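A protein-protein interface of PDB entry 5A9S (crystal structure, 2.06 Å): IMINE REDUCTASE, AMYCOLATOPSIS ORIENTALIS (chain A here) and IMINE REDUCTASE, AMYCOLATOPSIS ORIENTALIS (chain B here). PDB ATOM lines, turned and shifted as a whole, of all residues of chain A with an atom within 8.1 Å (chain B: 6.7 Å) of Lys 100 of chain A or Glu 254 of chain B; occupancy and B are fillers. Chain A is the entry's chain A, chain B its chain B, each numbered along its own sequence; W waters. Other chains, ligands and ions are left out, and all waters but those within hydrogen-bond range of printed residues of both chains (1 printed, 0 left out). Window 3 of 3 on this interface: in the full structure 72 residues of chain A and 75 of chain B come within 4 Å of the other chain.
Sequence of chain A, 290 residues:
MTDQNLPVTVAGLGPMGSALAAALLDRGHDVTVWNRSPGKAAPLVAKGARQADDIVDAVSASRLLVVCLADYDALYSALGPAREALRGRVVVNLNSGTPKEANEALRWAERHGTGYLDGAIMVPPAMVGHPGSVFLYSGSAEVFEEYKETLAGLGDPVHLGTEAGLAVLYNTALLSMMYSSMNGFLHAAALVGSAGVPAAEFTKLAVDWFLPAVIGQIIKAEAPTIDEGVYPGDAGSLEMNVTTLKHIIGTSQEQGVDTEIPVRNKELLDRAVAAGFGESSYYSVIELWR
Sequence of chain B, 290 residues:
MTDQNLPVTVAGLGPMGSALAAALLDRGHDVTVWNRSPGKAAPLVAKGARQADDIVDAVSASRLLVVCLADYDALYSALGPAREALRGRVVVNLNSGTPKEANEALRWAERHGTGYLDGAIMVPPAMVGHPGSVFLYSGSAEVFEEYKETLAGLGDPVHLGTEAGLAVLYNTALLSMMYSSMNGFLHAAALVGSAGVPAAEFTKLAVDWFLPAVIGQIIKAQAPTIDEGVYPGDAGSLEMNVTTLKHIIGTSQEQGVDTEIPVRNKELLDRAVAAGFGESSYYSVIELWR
Among the printed residues, merely in contact across the chains: Pro 99 of chain A with Thr 251 of chain B, Thr 98 of chain A with Thr 251 of chain B, Gly 97 of chain A with Thr 251 of chain B and Leu 169 of chain A with Gln 255 of chain B.
The side-chain hydroxyl (OG1) of Thr 98 of chain A is in hydrogen-bond range of the side-chain carboxylate (OE1) of Glu 254 of chain B, at 3.1 Å.
N of Lys 100 of chain A sits at hydrogen-bond distance from OE2 of Glu 254 of chain B.
OE2 of Glu 254 of chain B sits close to N of Pro 99 of chain A (3.2 Å).
N of Gly 97 of chain A is in hydrogen-bond range of OE1 of Glu 101 of chain A.
OG1 of Thr 98 of chain A sits at hydrogen-bond distance from N of Glu 101 of chain A.
OG of Ser 194 of chain B lies within hydrogen-bond range of NE2 of Gln 255 of chain B.
Of the 19 printed residues of chain A, 5 touch a printed residue of chain B.
Hydrophobic or aromatic side chains of chain A within 4 Å of the printed part of chain B: Pro 99 and Leu 169.
Among the printed residues, 7 pairs touch across the chains.
Lys 100 of chain A touches just one residue of chain B: Glu 254 (2.6 Å).
Of the printed residues of chain B, Pro 99 of chain A touches Thr 251 (3.3 Å) and Glu 254 (3.2 Å).
Of the printed residues of chain B, Gly 97 of chain A touches Thr 251 (3.8 Å).
Of the printed residues of chain A, Thr 251 of chain B touches Gly 97 (3.8 Å), Thr 98 (3.5 Å) and Pro 99 (3.3 Å).
Of the printed residues of chain A, Gln 255 of chain B touches Leu 169 (3.98 Å).
Of the printed residues of chain B, Leu 169 of chain A touches Gln 255.
Ser 96 of chain A touches none of the printed residues of chain B.
The nearest residue of chain B that does not touch Lys 100 of chain A is Gln 255 of chain B (5.9 Å).
The nearest residue of chain A that does not touch Glu 254 of chain B is Glu 101 of chain A (4.7 Å).
The nearest printed residue of chain A that does not touch Thr 251 of chain B is Leu 169 of chain A (4.01 Å).
Water W1 lies within hydrogen-bond range of the side-chain carboxylate of Glu 254 of chain B (2.6 Å), the side-chain amide oxygen of Gln 255 of chain B (2.7 Å) and the backbone NH of Lys 100 of chain A (3.4 Å).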
ATOM      1  N   TYR A  76       3.662   4.060  -2.240  1.00  0.00           N
ATOM      2  CA  TYR A  76       3.613   4.126  -3.704  1.00  0.00           C
ATOM      3  C   TYR A  76       4.431   5.297  -4.121  1.00  0.00           C
ATOM      4  O   TYR A  76       5.088   5.272  -5.145  1.00  0.00           O
ATOM      5  CB  TYR A  76       2.164   4.264  -4.207  1.00  0.00           C
ATOM      6  CG  TYR A  76       1.274   3.339  -3.467  1.00  0.00           C
ATOM      7  CD1 TYR A  76       1.626   1.994  -3.324  1.00  0.00           C
ATOM      8  CD2 TYR A  76       0.127   3.797  -2.814  1.00  0.00           C
ATOM      9  CE1 TYR A  76       0.856   1.133  -2.600  1.00  0.00           C
ATOM     10  CE2 TYR A  76      -0.659   2.912  -2.078  1.00  0.00           C
ATOM     11  CZ  TYR A  76      -0.271   1.582  -1.996  1.00  0.00           C
ATOM     12  OH  TYR A  76      -1.005   0.699  -1.280  1.00  0.00           O
ATOM     13  N   SER A  96       0.923  -0.434   6.968  1.00  0.00           N
ATOM     14  CA  SER A  96      -0.426  -0.149   6.423  1.00  0.00           C
ATOM     15  C   SER A  96      -1.409   0.202   7.557  1.00  0.00           C
ATOM     16  O   SER A  96      -1.329  -0.331   8.684  1.00  0.00           O
ATOM     17  CB  SER A  96      -1.025  -1.309   5.639  1.00  0.00           C
ATOM     18  OG  SER A  96      -0.101  -2.001   4.915  1.00  0.00           O
ATOM     19  N   GLY A  97      -2.338   1.087   7.193  1.00  0.00           N
ATOM     20  CA  GLY A  97      -3.375   1.567   8.057  1.00  0.00           C
ATOM     21  C   GLY A  97      -4.564   0.620   8.071  1.00  0.00           C
ATOM     22  O   GLY A  97      -5.047   0.352   9.178  1.00  0.00           O
ATOM     23  N   THR A  98      -5.075   0.165   6.902  1.00  0.00           N
ATOM     24  CA  THR A  98      -6.311  -0.640   6.844  1.00  0.00           C
ATOM     25  C   THR A  98      -6.090  -1.800   5.944  1.00  0.00           C
ATOM     26  O   THR A  98      -5.144  -1.764   5.123  1.00  0.00           O
ATOM     27  CB  THR A  98      -7.515   0.141   6.248  1.00  0.00           C
ATOM     28  OG1 THR A  98      -7.309   0.314   4.868  1.00  0.00           O
ATOM     29  CG2 THR A  98      -7.648   1.501   6.829  1.00  0.00           C
ATOM     30  N   PRO A  99      -6.994  -2.811   6.006  1.00  0.00           N
ATOM     31  CA  PRO A  99      -6.806  -3.965   5.137  1.00  0.00           C
ATOM     32  C   PRO A  99      -6.864  -3.653   3.652  1.00  0.00           C
ATOM     33  O   PRO A  99      -6.142  -4.241   2.872  1.00  0.00           O
ATOM     34  CB  PRO A  99      -7.986  -4.913   5.540  1.00  0.00           C
ATOM     35  CG  PRO A  99      -8.240  -4.541   6.960  1.00  0.00           C
ATOM     36  CD  PRO A  99      -8.017  -3.068   7.024  1.00  0.00           C
ATOM     37  N   LYS A 100      -7.773  -2.790   3.250  1.00  0.00           N
ATOM     38  CA  LYS A 100      -7.775  -2.330   1.868  1.00  0.00           C
ATOM     39  C   LYS A 100      -6.408  -1.786   1.422  1.00  0.00           C
ATOM     40  O   LYS A 100      -5.960  -2.108   0.320  1.00  0.00           O
ATOM     41  CB  LYS A 100      -8.882  -1.261   1.663  1.00  0.00           C
ATOM     42  CG  LYS A 100      -9.090  -0.755   0.242  1.00  0.00           C
ATOM     43  CD  LYS A 100     -10.099   0.399   0.237  1.00  0.00           C
ATOM     44  CE  LYS A 100     -10.654   0.722  -1.156  1.00  0.00           C
ATOM     45  N   GLU A 101      -5.761  -0.975   2.251  1.00  0.00           N
ATOM     46  CA  GLU A 101      -4.452  -0.422   1.896  1.00  0.00           C
ATOM     47  C   GLU A 101      -3.431  -1.532   1.766  1.00  0.00           C
ATOM     48  O   GLU A 101      -2.604  -1.473   0.871  1.00  0.00           O
ATOM     49  CB  GLU A 101      -3.941   0.612   2.901  1.00  0.00           C
ATOM     50  CG  GLU A 101      -4.815   1.855   3.000  1.00  0.00           C
ATOM     51  CD  GLU A 101      -4.398   2.795   4.117  1.00  0.00           C
ATOM     52  OE1 GLU A 101      -3.315   2.631   4.715  1.00  0.00           O
ATOM     53  OE2 GLU A 101      -5.136   3.727   4.390  1.00  0.00           O
ATOM     54  N   ALA A 102      -3.488  -2.542   2.651  1.00  0.00           N
ATOM     55  CA  ALA A 102      -2.618  -3.695   2.523  1.00  0.00           C
ATOM     56  C   ALA A 102      -2.821  -4.417   1.187  1.00  0.00           C
ATOM     57  O   ALA A 102      -1.859  -4.834   0.544  1.00  0.00           O
ATOM     58  CB  ALA A 102      -2.803  -4.660   3.657  1.00  0.00           C
ATOM     59  N   ASN A 103      -4.075  -4.579   0.806  1.00  0.00           N
ATOM     60  CA  ASN A 103      -4.404  -5.169  -0.489  1.00  0.00           C
ATOM     61  C   ASN A 103      -3.956  -4.353  -1.705  1.00  0.00           C
ATOM     62  O   ASN A 103      -3.498  -4.939  -2.680  1.00  0.00           O
ATOM     63  CB  ASN A 103      -5.907  -5.487  -0.542  1.00  0.00           C
ATOM     64  CG  ASN A 103      -6.246  -6.682   0.347  1.00  0.00           C
ATOM     65  OD1 ASN A 103      -5.364  -7.399   0.795  1.00  0.00           O
ATOM     66  ND2 ASN A 103      -7.490  -6.852   0.662  1.00  0.00           N
ATOM     67  N   GLU A 104      -4.079  -3.030  -1.648  1.00  0.00           N
ATOM     68  CA  GLU A 104      -3.552  -2.146  -2.685  1.00  0.00           C
ATOM     69  C   GLU A 104      -2.032  -2.267  -2.781  1.00  0.00           C
ATOM     70  O   GLU A 104      -1.504  -2.282  -3.855  1.00  0.00           O
ATOM     71  CB  GLU A 104      -3.899  -0.679  -2.436  1.00  0.00           C
ATOM     72  CG  GLU A 104      -5.306  -0.281  -2.880  1.00  0.00           C
ATOM     73  CD  GLU A 104      -5.872   0.990  -2.198  1.00  0.00           C
ATOM     74  OE1 GLU A 104      -5.124   1.715  -1.503  1.00  0.00           O
ATOM     75  OE2 GLU A 104      -7.086   1.266  -2.350  1.00  0.00           O
ATOM     76  N   ALA A 105      -1.344  -2.345  -1.655  1.00  0.00           N
ATOM     77  CA  ALA A 105       0.095  -2.485  -1.672  1.00  0.00           C
ATOM     78  C   ALA A 105       0.490  -3.822  -2.297  1.00  0.00           C
ATOM     79  O   ALA A 105       1.409  -3.853  -3.116  1.00  0.00           O
ATOM     80  CB  ALA A 105       0.696  -2.345  -0.272  1.00  0.00           C
ATOM     81  N   LEU A 106      -0.153  -4.909  -1.910  1.00  0.00           N
ATOM     82  CA  LEU A 106       0.055  -6.191  -2.569  1.00  0.00           C
ATOM     83  C   LEU A 106      -0.071  -6.114  -4.073  1.00  0.00           C
ATOM     84  O   LEU A 106       0.799  -6.608  -4.767  1.00  0.00           O
ATOM     85  CB  LEU A 106      -0.974  -7.204  -2.088  1.00  0.00           C
ATOM     86  CG  LEU A 106      -0.970  -8.593  -2.783  1.00  0.00           C
ATOM     87  CD1 LEU A 106       0.272  -9.430  -2.469  1.00  0.00           C
ATOM     88  CD2 LEU A 106      -2.234  -9.373  -2.510  1.00  0.00           C
ATOM     89  N   ARG A 107      -1.167  -5.522  -4.578  1.00  0.00           N
ATOM     90  CA  ARG A 107      -1.380  -5.404  -6.025  1.00  0.00           C
ATOM     91  C   ARG A 107      -0.245  -4.608  -6.642  1.00  0.00           C
ATOM     92  O   ARG A 107       0.310  -5.004  -7.653  1.00  0.00           O
ATOM     93  CB  ARG A 107      -2.723  -4.720  -6.372  1.00  0.00           C
ATOM     94  N   TYR A 116       5.580  -9.905  -1.442  1.00  0.00           N
ATOM     95  CA  TYR A 116       4.944  -9.012  -0.443  1.00  0.00           C
ATOM     96  C   TYR A 116       4.507  -9.711   0.851  1.00  0.00           C
ATOM     97  O   TYR A 116       3.805 -10.715   0.819  1.00  0.00           O
ATOM     98  CB  TYR A 116       3.736  -8.329  -1.052  1.00  0.00           C
ATOM     99  CG  TYR A 116       3.177  -7.234  -0.193  1.00  0.00           C
ATOM    100  CD1 TYR A 116       3.769  -5.972  -0.177  1.00  0.00           C
ATOM    101  CD2 TYR A 116       2.072  -7.445   0.607  1.00  0.00           C
ATOM    102  CE1 TYR A 116       3.251  -4.941   0.589  1.00  0.00           C
ATOM    103  CE2 TYR A 116       1.530  -6.425   1.373  1.00  0.00           C
ATOM    104  CZ  TYR A 116       2.114  -5.162   1.378  1.00  0.00           C
ATOM    105  OH  TYR A 116       1.612  -4.148   2.189  1.00  0.00           O
ATOM    106  N   ALA A 164      -3.223 -10.698   2.255  1.00  0.00           N
ATOM    107  CA  ALA A 164      -2.445  -9.514   2.598  1.00  0.00           C
ATOM    108  C   ALA A 164      -2.998  -8.718   3.779  1.00  0.00           C
ATOM    109  O   ALA A 164      -2.236  -8.278   4.606  1.00  0.00           O
ATOM    110  CB  ALA A 164      -2.323  -8.595   1.391  1.00  0.00           C
ATOM    111  N   GLY A 165      -4.312  -8.552   3.811  1.00  0.00           N
ATOM    112  CA  GLY A 165      -4.990  -7.747   4.779  1.00  0.00           C
ATOM    113  C   GLY A 165      -5.101  -8.269   6.204  1.00  0.00           C
ATOM    114  O   GLY A 165      -5.544  -7.547   7.064  1.00  0.00           O
ATOM    115  N   LEU A 166      -4.722  -9.495   6.474  1.00  0.00           N
ATOM    116  CA  LEU A 166      -4.998 -10.101   7.781  1.00  0.00           C
ATOM    117  C   LEU A 166      -4.253  -9.440   8.953  1.00  0.00           C
ATOM    118  O   LEU A 166      -4.829  -9.274  10.021  1.00  0.00           O
ATOM    119  CB  LEU A 166      -4.702 -11.563   7.731  1.00  0.00           C
ATOM    120  CG  LEU A 166      -5.686 -12.451   6.975  1.00  0.00           C
ATOM    121  CD1 LEU A 166      -5.022 -13.839   6.833  1.00  0.00           C
ATOM    122  CD2 LEU A 166      -7.066 -12.527   7.588  1.00  0.00           C
ATOM    123  N   VAL A 168      -3.082  -6.359   9.491  1.00  0.00           N
ATOM    124  CA  VAL A 168      -3.718  -5.094   9.846  1.00  0.00           C
ATOM    125  C   VAL A 168      -5.109  -5.324  10.461  1.00  0.00           C
ATOM    126  O   VAL A 168      -5.523  -4.611  11.362  1.00  0.00           O
ATOM    127  CB  VAL A 168      -3.745  -4.139   8.641  1.00  0.00           C
ATOM    128  CG1 VAL A 168      -4.422  -4.724   7.435  1.00  0.00           C
ATOM    129  CG2 VAL A 168      -4.441  -2.845   8.991  1.00  0.00           C
ATOM    130  N   LEU A 169      -5.825  -6.306   9.960  1.00  0.00           N
ATOM    131  CA  LEU A 169      -7.127  -6.618  10.512  1.00  0.00           C
ATOM    132  C   LEU A 169      -6.986  -7.067  11.983  1.00  0.00           C
ATOM    133  O   LEU A 169      -7.696  -6.585  12.824  1.00  0.00           O
ATOM    134  CB  LEU A 169      -7.848  -7.693   9.688  1.00  0.00           C
ATOM    135  CG  LEU A 169      -9.286  -8.025  10.143  1.00  0.00           C
ATOM    136  CD1 LEU A 169     -10.235  -6.856  10.040  1.00  0.00           C
ATOM    137  CD2 LEU A 169      -9.855  -9.147   9.324  1.00  0.00           C
ATOM    138  N   SER B 194     -15.843 -10.495  10.591  1.00  0.00           N
ATOM    139  CA  SER B 194     -16.309  -9.958   9.320  1.00  0.00           C
ATOM    140  C   SER B 194     -15.470 -10.438   8.146  1.00  0.00           C
ATOM    141  O   SER B 194     -15.956 -10.413   7.039  1.00  0.00           O
ATOM    142  CB  SER B 194     -16.309  -8.442   9.340  1.00  0.00           C
ATOM    143  OG  SER B 194     -14.956  -7.929   9.257  1.00  0.00           O
ATOM    144  N   ILE B 249     -11.238   2.879  12.867  1.00  0.00           N
ATOM    145  CA  ILE B 249     -12.566   3.291  12.356  1.00  0.00           C
ATOM    146  C   ILE B 249     -12.656   3.012  10.867  1.00  0.00           C
ATOM    147  O   ILE B 249     -13.626   2.393  10.405  1.00  0.00           O
ATOM    148  CB  ILE B 249     -12.808   4.781  12.627  1.00  0.00           C
ATOM    149  CG1 ILE B 249     -13.014   5.011  14.120  1.00  0.00           C
ATOM    150  CG2 ILE B 249     -14.024   5.307  11.839  1.00  0.00           C
ATOM    151  CD1 ILE B 249     -12.857   6.447  14.538  1.00  0.00           C
ATOM    152  N   GLY B 250     -11.606   3.388  10.115  1.00  0.00           N
ATOM    153  CA  GLY B 250     -11.532   3.109   8.687  1.00  0.00           C
ATOM    154  C   GLY B 250     -11.722   1.624   8.411  1.00  0.00           C
ATOM    155  O   GLY B 250     -12.459   1.235   7.445  1.00  0.00           O
ATOM    156  N   THR B 251     -11.030   0.788   9.203  1.00  0.00           N
ATOM    157  CA  THR B 251     -11.040  -0.636   9.028  1.00  0.00           C
ATOM    158  C   THR B 251     -12.409  -1.171   9.328  1.00  0.00           C
ATOM    159  O   THR B 251     -12.927  -2.017   8.600  1.00  0.00           O
ATOM    160  CB  THR B 251      -9.942  -1.353   9.856  1.00  0.00           C
ATOM    161  OG1 THR B 251      -8.629  -0.951   9.423  1.00  0.00           O
ATOM    162  CG2 THR B 251     -10.103  -2.855   9.776  1.00  0.00           C
ATOM    163  N   SER B 252     -13.027  -0.687  10.389  1.00  0.00           N
ATOM    164  CA  SER B 252     -14.378  -1.106  10.679  1.00  0.00           C
ATOM    165  C   SER B 252     -15.398  -0.769   9.552  1.00  0.00           C
ATOM    166  O   SER B 252     -16.257  -1.574   9.201  1.00  0.00           O
ATOM    167  CB  SER B 252     -14.872  -0.495  12.013  1.00  0.00           C
ATOM    168  OG  SER B 252     -14.148  -0.940  13.120  1.00  0.00           O
ATOM    169  N   GLN B 253     -15.331   0.445   9.037  1.00  0.00           N
ATOM    170  CA  GLN B 253     -16.168   0.873   7.877  1.00  0.00           C
ATOM    171  C   GLN B 253     -15.972  -0.013   6.651  1.00  0.00           C
ATOM    172  O   GLN B 253     -16.936  -0.569   6.134  1.00  0.00           O
ATOM    173  CB  GLN B 253     -15.839   2.319   7.479  1.00  0.00           C
ATOM    174  CG  GLN B 253     -16.412   3.334   8.438  1.00  0.00           C
ATOM    175  CD  GLN B 253     -15.881   4.732   8.210  1.00  0.00           C
ATOM    176  OE1 GLN B 253     -14.912   4.939   7.483  1.00  0.00           O
ATOM    177  NE2 GLN B 253     -16.473   5.693   8.888  1.00  0.00           N
ATOM    178  N   GLU B 254     -14.733  -0.223   6.227  1.00  0.00           N
ATOM    179  CA  GLU B 254     -14.507  -1.092   5.080  1.00  0.00           C
ATOM    180  C   GLU B 254     -14.940  -2.553   5.337  1.00  0.00           C
ATOM    181  O   GLU B 254     -15.366  -3.202   4.417  1.00  0.00           O
ATOM    182  CB  GLU B 254     -13.113  -0.858   4.464  1.00  0.00           C
ATOM    183  CG  GLU B 254     -11.952  -1.374   5.203  1.00  0.00           C
ATOM    184  CD  GLU B 254     -10.599  -0.915   4.620  1.00  0.00           C
ATOM    185  OE1 GLU B 254     -10.368   0.266   4.237  1.00  0.00           O
ATOM    186  OE2 GLU B 254      -9.701  -1.740   4.639  1.00  0.00           O
ATOM    187  N   GLN B 255     -14.928  -3.033   6.587  1.00  0.00           N
ATOM    188  CA  GLN B 255     -15.389  -4.404   6.925  1.00  0.00           C
ATOM    189  C   GLN B 255     -16.882  -4.520   7.185  1.00  0.00           C
ATOM    190  O   GLN B 255     -17.368  -5.627   7.396  1.00  0.00           O
ATOM    191  CB  GLN B 255     -14.638  -4.964   8.132  1.00  0.00           C
ATOM    192  CG  GLN B 255     -13.134  -5.182   7.890  1.00  0.00           C
ATOM    193  CD  GLN B 255     -12.846  -6.126   6.752  1.00  0.00           C
ATOM    194  OE1 GLN B 255     -12.164  -5.761   5.818  1.00  0.00           O
ATOM    195  NE2 GLN B 255     -13.365  -7.349   6.822  1.00  0.00           N
ATOM    196  N   GLY B 256     -17.614  -3.412   7.194  1.00  0.00           N
ATOM    197  CA  GLY B 256     -19.051  -3.448   7.441  1.00  0.00           C
ATOM    198  C   GLY B 256     -19.372  -3.661   8.905  1.00  0.00           C
ATOM    199  O   GLY B 256     -20.415  -4.184   9.215  1.00  0.00           O
ATOM    200  N   VAL B 257     -18.515  -3.205   9.832  1.00  0.00           N
ATOM    201  CA  VAL B 257     -18.746  -3.426  11.267  1.00  0.00           C
ATOM    202  C   VAL B 257     -19.036  -2.094  11.888  1.00  0.00           C
ATOM    203  O   VAL B 257     -18.421  -1.128  11.530  1.00  0.00           O
ATOM    204  CB  VAL B 257     -17.513  -4.137  11.928  1.00  0.00           C
ATOM    205  CG1 VAL B 257     -17.587  -4.165  13.454  1.00  0.00           C
ATOM    206  CG2 VAL B 257     -17.433  -5.556  11.387  1.00  0.00           C
HETATM  207  O   HOH W   1     -10.829  -4.058   4.154  1.00  0.00           O
